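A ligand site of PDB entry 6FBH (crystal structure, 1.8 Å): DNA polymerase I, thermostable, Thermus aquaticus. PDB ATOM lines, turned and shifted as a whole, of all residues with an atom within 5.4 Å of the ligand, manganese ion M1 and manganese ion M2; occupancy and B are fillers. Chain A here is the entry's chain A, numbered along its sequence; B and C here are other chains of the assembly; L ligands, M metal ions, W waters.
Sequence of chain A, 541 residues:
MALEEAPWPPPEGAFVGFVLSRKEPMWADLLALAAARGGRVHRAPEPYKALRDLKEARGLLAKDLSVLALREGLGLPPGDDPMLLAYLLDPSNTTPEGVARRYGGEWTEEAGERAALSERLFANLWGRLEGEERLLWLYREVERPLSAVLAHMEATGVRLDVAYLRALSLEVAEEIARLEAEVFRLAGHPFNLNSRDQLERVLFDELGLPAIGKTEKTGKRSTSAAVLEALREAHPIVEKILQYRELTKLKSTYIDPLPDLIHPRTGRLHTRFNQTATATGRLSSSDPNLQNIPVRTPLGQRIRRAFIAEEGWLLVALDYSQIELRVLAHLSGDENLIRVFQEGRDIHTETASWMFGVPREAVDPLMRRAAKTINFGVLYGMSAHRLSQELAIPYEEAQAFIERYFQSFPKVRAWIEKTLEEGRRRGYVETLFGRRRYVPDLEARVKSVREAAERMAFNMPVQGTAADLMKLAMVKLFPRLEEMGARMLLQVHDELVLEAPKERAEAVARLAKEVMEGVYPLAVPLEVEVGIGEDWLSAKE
The guanidinium group (NH2) of Arg 369 lies within hydrogen-bond range of a nitrogen (N4) of the ligand, at 2.7 Å. An oxygen (O8) of the ligand sits at hydrogen-bond distance from the backbone NH (N) of Glu 324, at 3.1 Å. An oxygen (O7) of the ligand lies within salt-bridge range of the side-chain amino group (NZ) of Lys 372, 2.8 Å away. N3 of DG 5 of chain C lies close to a nitrogen (N2) of the ligand, at 3.3 Å. A nitrogen (N2) of the ligand sits at hydrogen-bond distance from O2 of DC 4 of chain C (2.8 Å). An oxygen (O7) of the ligand is in salt-bridge range of the guanidinium group of Arg 368 (2.7 Å). An oxygen (O6) of the ligand is in hydrogen-bond range of a ring nitrogen (NE2) of His 348, 3.1 Å away. The guanidinium group (NH2) of Arg 282 sits at hydrogen-bond distance from an oxygen (O11) of the ligand. An oxygen (O4) of the ligand lies within hydrogen-bond range of the backbone NH (N) of Gln 322 (3.3 Å). An oxygen (O3) of the ligand sits close to the backbone NH of Ile 323, 3.2 Å away.
OG of Ser 321 lies within hydrogen-bond range of NE2 of Gln 322 (3.5 Å). OE1 of Glu 324 lies within hydrogen-bond range of OH of Tyr 380, at 2.5 Å. OD2 of Asp 346 is in salt-bridge range of NH2 of Arg 368 (2.7 Å). O of Arg 369 sits at hydrogen-bond distance from OG1 of Thr 373, 3.2 Å away. The guanidinium group of Arg 282 lies within salt-bridge range of the side-chain carboxylate of Glu 324 (3.9 Å). N of His 348 is in hydrogen-bond range of OD1 of Asp 346 (2.9 Å). NZ of Lys 540 sits close to OD2 of Asp 319. O2 of DC 12 of chain B is in hydrogen-bond range of NH1 of Arg 282 (2.9 Å).
Residues that only touch the ligand: Phe 376 (3.3 Å), Tyr 380 (3.4 Å) and Ser 321 (3.7 Å). Hydrophobic or aromatic side chains within 4 Å of the ligand: Ile 323, His 348, Phe 376 and Tyr 380. Within 4 Å of the ligand: Arg 282, Asp 319, Tyr 320, Ser 321, Gln 322, Ile 323, Glu 324, His 348, Arg 368, Arg 369, Lys 372, Phe 376, Tyr 380, Asp 494, DC 12 of chain B, DC 4 of chain C and DG 5 of chain C. The nearest printed residue that does not touch the ligand is Thr 373 (4.003 Å).
Three residues have an atom within 4 Å of manganese ion M1: Asp 319, Asp 494 and DC 12 of chain B.
Within 4 Å of manganese ion M2: Asp 319, Tyr 320 and Asp 494. The nearest printed residue that does not touch manganese ion M2 is Gln 322 (4.3 Å).
Manganese ion M1 is bound by water W2 (1.8 Å), the side-chain carboxylate (OD1) of Asp 494 (2.1 Å), water W1 (2.1 Å), an oxygen (O2) of the ligand (2.2 Å), the side-chain carboxylate (OD2) of Asp 319 (2.2 Å) and O3' of DC 12 of chain B (2.3 Å).
Manganese ion M2 is bound by O10 of the ligand (2.0 Å), OD2 of Asp 494 (2.1 Å), OD1 of Asp 319 (2.2 Å), O of Tyr 320 (2.2 Å), O3 of the ligand (2.2 Å) and O2 of the ligand (2.3 Å). Manganese ion M2 has six donor atoms within binding distance.
Water W1 lies within hydrogen-bond range of OE1 of Glu 495 (2.6 Å) and O of Val 492 (3.3 Å). Water W7 lies within hydrogen-bond range of OP2 of DC 12 of chain B (2.7 Å), NH2 of Arg 369 (2.8 Å) and O5 of the ligand (2.9 Å). Water W3 lies within hydrogen-bond range of the side-chain carboxylate (OE1) of Glu 324 (2.8 Å), a nitrogen (N3) of the ligand (3.0 Å) and the side-chain amide nitrogen (ND2) of Asn 459 (3.1 Å). Water W4 lies within hydrogen-bond range of the side-chain carboxylate of Glu 324 (2.7 Å), the guanidinium group of Arg 282 (2.8 Å) and an oxygen (O11) of the ligand (3.5 Å).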
ATOM      1  N   ARG A 282       6.922 -30.020  -7.779  1.00  0.00           N
ATOM      2  CA  ARG A 282       5.678 -30.363  -7.091  1.00  0.00           C
ATOM      3  C   ARG A 282       4.556 -30.632  -8.085  1.00  0.00           C
ATOM      4  O   ARG A 282       4.545 -30.116  -9.206  1.00  0.00           O
ATOM      5  CB  ARG A 282       5.260 -29.230  -6.156  1.00  0.00           C
ATOM      6  CG  ARG A 282       5.963 -29.210  -4.839  1.00  0.00           C
ATOM      7  CD  ARG A 282       5.358 -28.168  -3.969  1.00  0.00           C
ATOM      8  NE  ARG A 282       5.713 -28.310  -2.576  1.00  0.00           N
ATOM      9  CZ  ARG A 282       5.104 -27.675  -1.591  1.00  0.00           C
ATOM     10  NH1 ARG A 282       4.107 -26.824  -1.859  1.00  0.00           N
ATOM     11  NH2 ARG A 282       5.479 -27.890  -0.335  1.00  0.00           N
ATOM     12  N   ASP A 319       2.480 -38.655   6.436  1.00  0.00           N
ATOM     13  CA  ASP A 319       3.013 -37.317   6.245  1.00  0.00           C
ATOM     14  C   ASP A 319       4.445 -37.290   6.749  1.00  0.00           C
ATOM     15  O   ASP A 319       4.689 -37.543   7.936  1.00  0.00           O
ATOM     16  CB  ASP A 319       2.139 -36.291   6.961  1.00  0.00           C
ATOM     17  CG  ASP A 319       2.607 -34.856   6.712  1.00  0.00           C
ATOM     18  OD1 ASP A 319       3.748 -34.545   7.092  1.00  0.00           O
ATOM     19  OD2 ASP A 319       1.827 -34.086   6.130  1.00  0.00           O
ATOM     20  N   TYR A 320       5.391 -36.997   5.858  1.00  0.00           N
ATOM     21  CA  TYR A 320       6.792 -36.895   6.242  1.00  0.00           C
ATOM     22  C   TYR A 320       6.978 -35.852   7.331  1.00  0.00           C
ATOM     23  O   TYR A 320       6.362 -34.777   7.323  1.00  0.00           O
ATOM     24  CB  TYR A 320       7.649 -36.525   5.042  1.00  0.00           C
ATOM     25  CG  TYR A 320       7.889 -37.627   4.034  1.00  0.00           C
ATOM     26  CD1 TYR A 320       8.778 -38.662   4.313  1.00  0.00           C
ATOM     27  CD2 TYR A 320       7.263 -37.621   2.804  1.00  0.00           C
ATOM     28  CE1 TYR A 320       9.017 -39.681   3.383  1.00  0.00           C
ATOM     29  CE2 TYR A 320       7.487 -38.612   1.877  1.00  0.00           C
ATOM     30  CZ  TYR A 320       8.357 -39.637   2.168  1.00  0.00           C
ATOM     31  OH  TYR A 320       8.581 -40.627   1.241  1.00  0.00           O
ATOM     32  N   SER A 321       7.849 -36.176   8.287  1.00  0.00           N
ATOM     33  CA  SER A 321       8.180 -35.277   9.375  1.00  0.00           C
ATOM     34  C   SER A 321       9.194 -34.237   8.911  1.00  0.00           C
ATOM     35  O   SER A 321      10.228 -34.591   8.332  1.00  0.00           O
ATOM     36  CB  SER A 321       8.722 -36.089  10.555  1.00  0.00           C
ATOM     37  OG  SER A 321       9.127 -35.248  11.615  1.00  0.00           O
ATOM     38  N   GLN A 322       8.873 -32.962   9.137  1.00  0.00           N
ATOM     39  CA  GLN A 322       9.827 -31.834   8.969  1.00  0.00           C
ATOM     40  C   GLN A 322      10.619 -31.961   7.670  1.00  0.00           C
ATOM     41  O   GLN A 322      11.851 -31.859   7.647  1.00  0.00           O
ATOM     42  CB  GLN A 322      10.791 -31.757  10.152  1.00  0.00           C
ATOM     43  CG  GLN A 322      10.147 -31.782  11.532  1.00  0.00           C
ATOM     44  CD  GLN A 322      11.171 -31.894  12.646  1.00  0.00           C
ATOM     45  OE1 GLN A 322      11.813 -30.914  13.016  1.00  0.00           O
ATOM     46  NE2 GLN A 322      11.330 -33.103  13.183  1.00  0.00           N
ATOM     47  N   ILE A 323       9.901 -32.185   6.573  1.00  0.00           N
ATOM     48  CA  ILE A 323      10.536 -32.805   5.410  1.00  0.00           C
ATOM     49  C   ILE A 323      11.595 -31.887   4.812  1.00  0.00           C
ATOM     50  O   ILE A 323      12.722 -32.327   4.556  1.00  0.00           O
ATOM     51  CB  ILE A 323       9.471 -33.233   4.368  1.00  0.00           C
ATOM     52  CG1 ILE A 323      10.150 -33.931   3.195  1.00  0.00           C
ATOM     53  CG2 ILE A 323       8.659 -32.052   3.845  1.00  0.00           C
ATOM     54  CD1 ILE A 323      10.902 -35.169   3.561  1.00  0.00           C
ATOM     55  N   GLU A 324      11.265 -30.617   4.546  1.00  0.00           N
ATOM     56  CA  GLU A 324      12.266 -29.773   3.895  1.00  0.00           C
ATOM     57  C   GLU A 324      13.457 -29.513   4.824  1.00  0.00           C
ATOM     58  O   GLU A 324      14.576 -29.310   4.343  1.00  0.00           O
ATOM     59  CB  GLU A 324      11.627 -28.465   3.373  1.00  0.00           C
ATOM     60  CG  GLU A 324      10.914 -28.667   2.030  1.00  0.00           C
ATOM     61  CD  GLU A 324      10.301 -27.409   1.444  1.00  0.00           C
ATOM     62  OE1 GLU A 324      10.880 -26.327   1.642  1.00  0.00           O
ATOM     63  OE2 GLU A 324       9.220 -27.495   0.799  1.00  0.00           O
ATOM     64  N   LEU A 325      13.255 -29.572   6.145  1.00  0.00           N
ATOM     65  CA  LEU A 325      14.412 -29.444   7.046  1.00  0.00           C
ATOM     66  C   LEU A 325      15.305 -30.680   6.977  1.00  0.00           C
ATOM     67  O   LEU A 325      16.544 -30.555   7.025  1.00  0.00           O
ATOM     68  CB  LEU A 325      13.956 -29.179   8.489  1.00  0.00           C
ATOM     69  CG  LEU A 325      13.276 -27.819   8.739  1.00  0.00           C
ATOM     70  CD1 LEU A 325      12.915 -27.618  10.223  1.00  0.00           C
ATOM     71  CD2 LEU A 325      14.170 -26.674   8.255  1.00  0.00           C
ATOM     72  N   ASP A 346      12.548 -32.092  17.318  1.00  0.00           N
ATOM     73  CA  ASP A 346      11.509 -31.491  16.497  1.00  0.00           C
ATOM     74  C   ASP A 346      11.688 -29.980  16.547  1.00  0.00           C
ATOM     75  O   ASP A 346      11.419 -29.349  17.577  1.00  0.00           O
ATOM     76  CB  ASP A 346      10.112 -31.886  16.990  1.00  0.00           C
ATOM     77  CG  ASP A 346       9.010 -31.421  16.046  1.00  0.00           C
ATOM     78  OD1 ASP A 346       9.150 -30.343  15.432  1.00  0.00           O
ATOM     79  OD2 ASP A 346       7.998 -32.150  15.897  1.00  0.00           O
ATOM     80  N   HIS A 348      10.056 -27.669  14.841  1.00  0.00           N
ATOM     81  CA  HIS A 348       8.787 -26.950  14.905  1.00  0.00           C
ATOM     82  C   HIS A 348       8.297 -26.846  16.343  1.00  0.00           C
ATOM     83  O   HIS A 348       7.841 -25.791  16.783  1.00  0.00           O
ATOM     84  CB  HIS A 348       7.734 -27.633  14.019  1.00  0.00           C
ATOM     85  CG  HIS A 348       8.105 -27.672  12.563  1.00  0.00           C
ATOM     86  ND1 HIS A 348       8.808 -26.669  11.944  1.00  0.00           N
ATOM     87  CD2 HIS A 348       7.862 -28.613  11.613  1.00  0.00           C
ATOM     88  CE1 HIS A 348       8.975 -26.972  10.664  1.00  0.00           C
ATOM     89  NE2 HIS A 348       8.415 -28.154  10.442  1.00  0.00           N
ATOM     90  N   ARG A 368       2.094 -25.254  16.838  1.00  0.00           N
ATOM     91  CA  ARG A 368       3.140 -25.865  16.030  1.00  0.00           C
ATOM     92  C   ARG A 368       3.075 -25.361  14.585  1.00  0.00           C
ATOM     93  O   ARG A 368       4.111 -25.126  13.958  1.00  0.00           O
ATOM     94  CB  ARG A 368       3.017 -27.390  16.089  1.00  0.00           C
ATOM     95  CG  ARG A 368       4.269 -28.141  15.676  1.00  0.00           C
ATOM     96  CD  ARG A 368       4.206 -29.656  15.983  1.00  0.00           C
ATOM     97  NE  ARG A 368       5.379 -30.334  15.436  1.00  0.00           N
ATOM     98  CZ  ARG A 368       5.516 -30.658  14.151  1.00  0.00           C
ATOM     99  NH1 ARG A 368       4.555 -30.375  13.284  1.00  0.00           N
ATOM    100  NH2 ARG A 368       6.614 -31.254  13.733  1.00  0.00           N
ATOM    101  N   ARG A 369       1.859 -25.179  14.058  1.00  0.00           N
ATOM    102  CA  ARG A 369       1.718 -24.636  12.709  1.00  0.00           C
ATOM    103  C   ARG A 369       2.327 -23.241  12.626  1.00  0.00           C
ATOM    104  O   ARG A 369       3.045 -22.919  11.670  1.00  0.00           O
ATOM    105  CB  ARG A 369       0.236 -24.611  12.314  1.00  0.00           C
ATOM    106  CG  ARG A 369      -0.039 -24.919  10.843  1.00  0.00           C
ATOM    107  CD  ARG A 369       0.559 -23.881   9.885  1.00  0.00           C
ATOM    108  NE  ARG A 369       1.239 -24.518   8.745  1.00  0.00           N
ATOM    109  CZ  ARG A 369       2.137 -23.912   7.973  1.00  0.00           C
ATOM    110  NH1 ARG A 369       2.506 -22.658   8.206  1.00  0.00           N
ATOM    111  NH2 ARG A 369       2.694 -24.571   6.960  1.00  0.00           N
ATOM    112  N   LYS A 372       5.896 -23.574  12.461  1.00  0.00           N
ATOM    113  CA  LYS A 372       6.247 -24.040  11.133  1.00  0.00           C
ATOM    114  C   LYS A 372       6.480 -22.858  10.182  1.00  0.00           C
ATOM    115  O   LYS A 372       7.490 -22.786   9.474  1.00  0.00           O
ATOM    116  CB  LYS A 372       5.117 -24.935  10.627  1.00  0.00           C
ATOM    117  CG  LYS A 372       5.430 -25.750   9.429  1.00  0.00           C
ATOM    118  CD  LYS A 372       4.269 -26.689   9.156  1.00  0.00           C
ATOM    119  CE  LYS A 372       4.235 -27.851  10.179  1.00  0.00           C
ATOM    120  NZ  LYS A 372       3.128 -28.798   9.890  1.00  0.00           N
ATOM    121  N   THR A 373       5.539 -21.907  10.160  1.00  0.00           N
ATOM    122  CA  THR A 373       5.670 -20.768   9.257  1.00  0.00           C
ATOM    123  C   THR A 373       6.897 -19.934   9.588  1.00  0.00           C
ATOM    124  O   THR A 373       7.570 -19.423   8.674  1.00  0.00           O
ATOM    125  CB  THR A 373       4.404 -19.928   9.345  1.00  0.00           C
ATOM    126  OG1 THR A 373       3.261 -20.780   9.263  1.00  0.00           O
ATOM    127  CG2 THR A 373       4.362 -18.903   8.226  1.00  0.00           C
ATOM    128  N   PHE A 376      10.212 -21.884   8.314  1.00  0.00           N
ATOM    129  CA  PHE A 376      10.457 -21.807   6.890  1.00  0.00           C
ATOM    130  C   PHE A 376      10.504 -20.358   6.428  1.00  0.00           C
ATOM    131  O   PHE A 376      11.309 -20.019   5.563  1.00  0.00           O
ATOM    132  CB  PHE A 376       9.398 -22.647   6.139  1.00  0.00           C
ATOM    133  CG  PHE A 376       9.582 -24.124   6.362  1.00  0.00           C
ATOM    134  CD1 PHE A 376      10.727 -24.750   5.924  1.00  0.00           C
ATOM    135  CD2 PHE A 376       8.643 -24.884   7.057  1.00  0.00           C
ATOM    136  CE1 PHE A 376      10.936 -26.106   6.149  1.00  0.00           C
ATOM    137  CE2 PHE A 376       8.844 -26.241   7.277  1.00  0.00           C
ATOM    138  CZ  PHE A 376       9.988 -26.847   6.816  1.00  0.00           C
ATOM    139  N   GLY A 377       9.712 -19.492   7.030  1.00  0.00           N
ATOM    140  CA  GLY A 377       9.820 -18.076   6.691  1.00  0.00           C
ATOM    141  C   GLY A 377      11.241 -17.580   6.845  1.00  0.00           C
ATOM    142  O   GLY A 377      11.807 -16.983   5.930  1.00  0.00           O
ATOM    143  N   TYR A 380      13.938 -19.246   4.274  1.00  0.00           N
ATOM    144  CA  TYR A 380      13.893 -18.830   2.886  1.00  0.00           C
ATOM    145  C   TYR A 380      13.903 -17.322   2.721  1.00  0.00           C
ATOM    146  O   TYR A 380      13.597 -16.828   1.624  1.00  0.00           O
ATOM    147  CB  TYR A 380      12.652 -19.434   2.217  1.00  0.00           C
ATOM    148  CG  TYR A 380      12.738 -20.936   2.116  1.00  0.00           C
ATOM    149  CD1 TYR A 380      13.802 -21.541   1.465  1.00  0.00           C
ATOM    150  CD2 TYR A 380      11.756 -21.762   2.664  1.00  0.00           C
ATOM    151  CE1 TYR A 380      13.888 -22.933   1.352  1.00  0.00           C
ATOM    152  CE2 TYR A 380      11.846 -23.153   2.564  1.00  0.00           C
ATOM    153  CZ  TYR A 380      12.923 -23.728   1.908  1.00  0.00           C
ATOM    154  OH  TYR A 380      13.022 -25.099   1.790  1.00  0.00           O
ATOM    155  N   ASN A 459      15.276 -21.898  -2.768  1.00  0.00           N
ATOM    156  CA  ASN A 459      14.145 -22.714  -2.322  1.00  0.00           C
ATOM    157  C   ASN A 459      13.998 -23.959  -3.185  1.00  0.00           C
ATOM    158  O   ASN A 459      13.736 -25.055  -2.658  1.00  0.00           O
ATOM    159  CB  ASN A 459      12.869 -21.878  -2.342  1.00  0.00           C
ATOM    160  CG  ASN A 459      11.599 -22.696  -2.106  1.00  0.00           C
ATOM    161  OD1 ASN A 459      10.940 -23.124  -3.056  1.00  0.00           O
ATOM    162  ND2 ASN A 459      11.212 -22.874  -0.850  1.00  0.00           N
ATOM    163  N   VAL A 492      -0.742 -34.656  -1.008  1.00  0.00           N
ATOM    164  CA  VAL A 492      -0.720 -33.260  -0.588  1.00  0.00           C
ATOM    165  C   VAL A 492       0.729 -32.869  -0.305  1.00  0.00           C
ATOM    166  O   VAL A 492       1.083 -32.519   0.823  1.00  0.00           O
ATOM    167  CB  VAL A 492      -1.626 -33.031   0.638  1.00  0.00           C
ATOM    168  CG1 VAL A 492      -1.835 -31.561   0.866  1.00  0.00           C
ATOM    169  CG2 VAL A 492      -2.969 -33.726   0.425  1.00  0.00           C
ATOM    170  N   ASP A 494       3.694 -33.621   0.752  1.00  0.00           N
ATOM    171  CA  ASP A 494       4.525 -34.554   1.510  1.00  0.00           C
ATOM    172  C   ASP A 494       3.650 -35.559   2.263  1.00  0.00           C
ATOM    173  O   ASP A 494       4.097 -36.151   3.255  1.00  0.00           O
ATOM    174  CB  ASP A 494       5.486 -33.833   2.459  1.00  0.00           C
ATOM    175  CG  ASP A 494       4.818 -33.342   3.720  1.00  0.00           C
ATOM    176  OD1 ASP A 494       3.644 -32.964   3.623  1.00  0.00           O
ATOM    177  OD2 ASP A 494       5.483 -33.330   4.790  1.00  0.00           O
ATOM    178  N   GLU A 495       2.440 -35.766   1.788  1.00  0.00           N
ATOM    179  CA  GLU A 495       1.431 -36.559   2.469  1.00  0.00           C
ATOM    180  C   GLU A 495       0.702 -37.393   1.440  1.00  0.00           C
ATOM    181  O   GLU A 495       0.502 -36.956   0.298  1.00  0.00           O
ATOM    182  CB  GLU A 495       0.444 -35.656   3.239  1.00  0.00           C
ATOM    183  CG  GLU A 495      -0.823 -36.366   3.735  1.00  0.00           C
ATOM    184  CD  GLU A 495      -1.808 -35.417   4.392  1.00  0.00           C
ATOM    185  OE1 GLU A 495      -1.483 -34.199   4.476  1.00  0.00           O
ATOM    186  OE2 GLU A 495      -2.892 -35.881   4.814  1.00  0.00           O
ATOM    187  N   LYS A 540      -5.274 -38.018  10.599  1.00  0.00           N
ATOM    188  CA  LYS A 540      -4.074 -37.219  10.814  1.00  0.00           C
ATOM    189  C   LYS A 540      -3.736 -37.029  12.286  1.00  0.00           C
ATOM    190  O   LYS A 540      -2.927 -36.153  12.609  1.00  0.00           O
ATOM    191  CB  LYS A 540      -4.192 -35.853  10.140  1.00  0.00           C
ATOM    192  CG  LYS A 540      -4.177 -35.899   8.606  1.00  0.00           C
ATOM    193  CD  LYS A 540      -3.461 -34.696   8.004  1.00  0.00           C
ATOM    194  CE  LYS A 540      -1.946 -34.826   8.157  1.00  0.00           C
ATOM    195  NZ  LYS A 540      -1.190 -33.702   7.531  1.00  0.00           N
ATOM    196  P    DC B  12      -1.830 -28.365   5.458  1.00  0.00           P
ATOM    197  OP1  DC B  12      -2.146 -29.726   5.946  1.00  0.00           O
ATOM    198  OP2  DC B  12      -1.531 -27.252   6.391  1.00  0.00           O
ATOM    199  O5'  DC B  12      -0.591 -28.454   4.443  1.00  0.00           O
ATOM    200  C5'  DC B  12      -0.595 -29.457   3.394  1.00  0.00           C
ATOM    201  C4'  DC B  12       0.626 -29.322   2.515  1.00  0.00           C
ATOM    202  O4'  DC B  12       0.600 -28.031   1.867  1.00  0.00           O
ATOM    203  C3'  DC B  12       1.946 -29.352   3.277  1.00  0.00           C
ATOM    204  O3'  DC B  12       2.444 -30.631   3.337  1.00  0.00           O
ATOM    205  C2'  DC B  12       2.865 -28.457   2.457  1.00  0.00           C
ATOM    206  C1'  DC B  12       1.917 -27.529   1.727  1.00  0.00           C
ATOM    207  N1   DC B  12       1.928 -26.141   2.232  1.00  0.00           N
ATOM    208  C2   DC B  12       2.745 -25.213   1.619  1.00  0.00           C
ATOM    209  O2   DC B  12       3.485 -25.601   0.702  1.00  0.00           O
ATOM    210  N3   DC B  12       2.749 -23.928   2.064  1.00  0.00           N
ATOM    211  C4   DC B  12       1.938 -23.572   3.056  1.00  0.00           C
ATOM    212  N4   DC B  12       1.966 -22.296   3.458  1.00  0.00           N
ATOM    213  C5   DC B  12       1.075 -24.500   3.691  1.00  0.00           C
ATOM    214  C6   DC B  12       1.102 -25.774   3.251  1.00  0.00           C
ATOM    215  P    DC C   4       9.391 -10.885   3.400  1.00  0.00           P
ATOM    216  OP1  DC C   4       7.950 -10.610   3.263  1.00  0.00           O
ATOM    217  OP2  DC C   4      10.152 -10.317   4.528  1.00  0.00           O
ATOM    218  O5'  DC C   4       9.616 -12.466   3.453  1.00  0.00           O
ATOM    219  C5'  DC C   4       9.140 -13.250   2.389  1.00  0.00           C
ATOM    220  C4'  DC C   4      10.004 -14.471   2.203  1.00  0.00           C
ATOM    221  O4'  DC C   4       9.968 -15.276   3.403  1.00  0.00           O
ATOM    222  C3'  DC C   4       9.558 -15.376   1.076  1.00  0.00           C
ATOM    223  O3'  DC C   4      10.150 -14.986  -0.119  1.00  0.00           O
ATOM    224  C2'  DC C   4      10.031 -16.753   1.555  1.00  0.00           C
ATOM    225  C1'  DC C   4       9.844 -16.644   3.064  1.00  0.00           C
ATOM    226  N1   DC C   4       8.523 -17.147   3.531  1.00  0.00           N
ATOM    227  C2   DC C   4       8.281 -18.521   3.457  1.00  0.00           C
ATOM    228  O2   DC C   4       9.166 -19.238   3.006  1.00  0.00           O
ATOM    229  N3   DC C   4       7.108 -19.008   3.900  1.00  0.00           N
ATOM    230  C4   DC C   4       6.187 -18.202   4.388  1.00  0.00           C
ATOM    231  N4   DC C   4       5.040 -18.738   4.811  1.00  0.00           N
ATOM    232  C5   DC C   4       6.396 -16.769   4.455  1.00  0.00           C
ATOM    233  C6   DC C   4       7.574 -16.301   4.025  1.00  0.00           C
ATOM    234  P    DG C   5       9.278 -14.925  -1.469  1.00  0.00           P
ATOM    235  OP1  DG C   5      10.175 -14.256  -2.436  1.00  0.00           O
ATOM    236  OP2  DG C   5       7.907 -14.454  -1.185  1.00  0.00           O
ATOM    237  O5'  DG C   5       9.137 -16.447  -1.929  1.00  0.00           O
ATOM    238  C5'  DG C   5      10.264 -17.116  -2.456  1.00  0.00           C
ATOM    239  C4'  DG C   5      10.039 -18.610  -2.507  1.00  0.00           C
ATOM    240  O4'  DG C   5       9.698 -19.084  -1.178  1.00  0.00           O
ATOM    241  C3'  DG C   5       8.901 -19.086  -3.384  1.00  0.00           C
ATOM    242  O3'  DG C   5       9.318 -19.220  -4.747  1.00  0.00           O
ATOM    243  C2'  DG C   5       8.553 -20.433  -2.754  1.00  0.00           C
ATOM    244  C1'  DG C   5       8.826 -20.186  -1.272  1.00  0.00           C
ATOM    245  N9   DG C   5       7.625 -19.893  -0.499  1.00  0.00           N
ATOM    246  C8   DG C   5       7.244 -18.681   0.036  1.00  0.00           C
ATOM    247  N7   DG C   5       6.132 -18.737   0.724  1.00  0.00           N
ATOM    248  C5   DG C   5       5.759 -20.088   0.615  1.00  0.00           C
ATOM    249  C6   DG C   5       4.633 -20.771   1.141  1.00  0.00           C
ATOM    250  O6   DG C   5       3.714 -20.329   1.837  1.00  0.00           O
ATOM    251  N1   DG C   5       4.651 -22.123   0.810  1.00  0.00           N
ATOM    252  C2   DG C   5       5.625 -22.735   0.054  1.00  0.00           C
ATOM    253  N2   DG C   5       5.473 -24.050  -0.176  1.00  0.00           N
ATOM    254  N3   DG C   5       6.681 -22.114  -0.442  1.00  0.00           N
ATOM    255  C4   DG C   5       6.673 -20.793  -0.127  1.00  0.00           C
HETATM  256  N1  LIG L   1       6.572 -21.748   3.806  1.00  0.00           N
HETATM  257  C1  LIG L   1       7.399 -22.469   2.995  1.00  0.00           C
HETATM  258  N2  LIG L   1       8.349 -21.797   2.352  1.00  0.00           N
HETATM  259  N3  LIG L   1       7.304 -23.790   2.830  1.00  0.00           N
HETATM  260  C2  LIG L   1       6.297 -24.331   3.543  1.00  0.00           C
HETATM  261  C3  LIG L   1       5.397 -23.694   4.350  1.00  0.00           C
HETATM  262  C4  LIG L   1       5.523 -22.261   4.530  1.00  0.00           C
HETATM  263  O1  LIG L   1       4.846 -21.537   5.251  1.00  0.00           O
HETATM  264  N4  LIG L   1       4.487 -24.598   4.880  1.00  0.00           N
HETATM  265  C5  LIG L   1       4.855 -25.749   4.383  1.00  0.00           C
HETATM  266  N5  LIG L   1       5.964 -25.656   3.591  1.00  0.00           N
HETATM  267  P1  LIG L   1       4.046 -29.868   6.375  1.00  0.00           P
HETATM  268  P2  LIG L   1       6.518 -30.367   7.881  1.00  0.00           P
HETATM  269  P3  LIG L   1       5.438 -31.858  10.071  1.00  0.00           P
HETATM  270  C6  LIG L   1       6.769 -26.760   3.055  1.00  0.00           C
HETATM  271  O2  LIG L   1       3.782 -31.288   6.177  1.00  0.00           O
HETATM  272  O3  LIG L   1       6.796 -31.465   6.973  1.00  0.00           O
HETATM  273  O4  LIG L   1       6.263 -32.583  11.073  1.00  0.00           O
HETATM  274  C7  LIG L   1       7.948 -27.112   3.971  1.00  0.00           C
HETATM  275  O5  LIG L   1       2.730 -29.172   6.744  1.00  0.00           O
HETATM  276  O6  LIG L   1       7.784 -29.436   7.745  1.00  0.00           O
HETATM  277  O7  LIG L   1       4.212 -31.230  10.704  1.00  0.00           O
HETATM  278  C8  LIG L   1       7.453 -28.341   4.736  1.00  0.00           C
HETATM  279  O8  LIG L   1       8.551 -29.185   5.069  1.00  0.00           O
HETATM  280  N6  LIG L   1       5.133 -29.606   7.543  1.00  0.00           N
HETATM  281  O9  LIG L   1       6.364 -30.737   9.423  1.00  0.00           O
HETATM  282  O10 LIG L   1       4.982 -32.696   8.848  1.00  0.00           O
HETATM  283  C9  LIG L   1       6.560 -29.012   3.698  1.00  0.00           C
HETATM  284  O11 LIG L   1       5.944 -27.919   2.986  1.00  0.00           O
HETATM  285  C10 LIG L   1       5.512 -29.942   4.234  1.00  0.00           C
HETATM  286  O12 LIG L   1       4.594 -29.214   5.064  1.00  0.00           O
HETATM  287 MN    MN M   1       2.270 -32.260   4.992  1.00  0.00          MN
HETATM  288 MN    MN M   2       5.217 -32.977   6.867  1.00  0.00          MN
HETATM  289  O   HOH W   1       0.458 -32.538   4.015  1.00  0.00           O
HETATM  290  O   HOH W   2       1.156 -31.440   6.159  1.00  0.00           O
HETATM  291  O   HOH W   3       8.995 -24.591   0.474  1.00  0.00           O
HETATM  292  O   HOH W   4       7.602 -29.569   0.404  1.00  0.00           O
HETATM  293  O   HOH W   5       4.148 -35.244   9.885  1.00  0.00           O
HETATM  294  O   HOH W   6       1.909 -32.157   8.846  1.00  0.00           O
HETATM  295  O   HOH W   7       1.063 -26.818   6.821  1.00  0.00           O
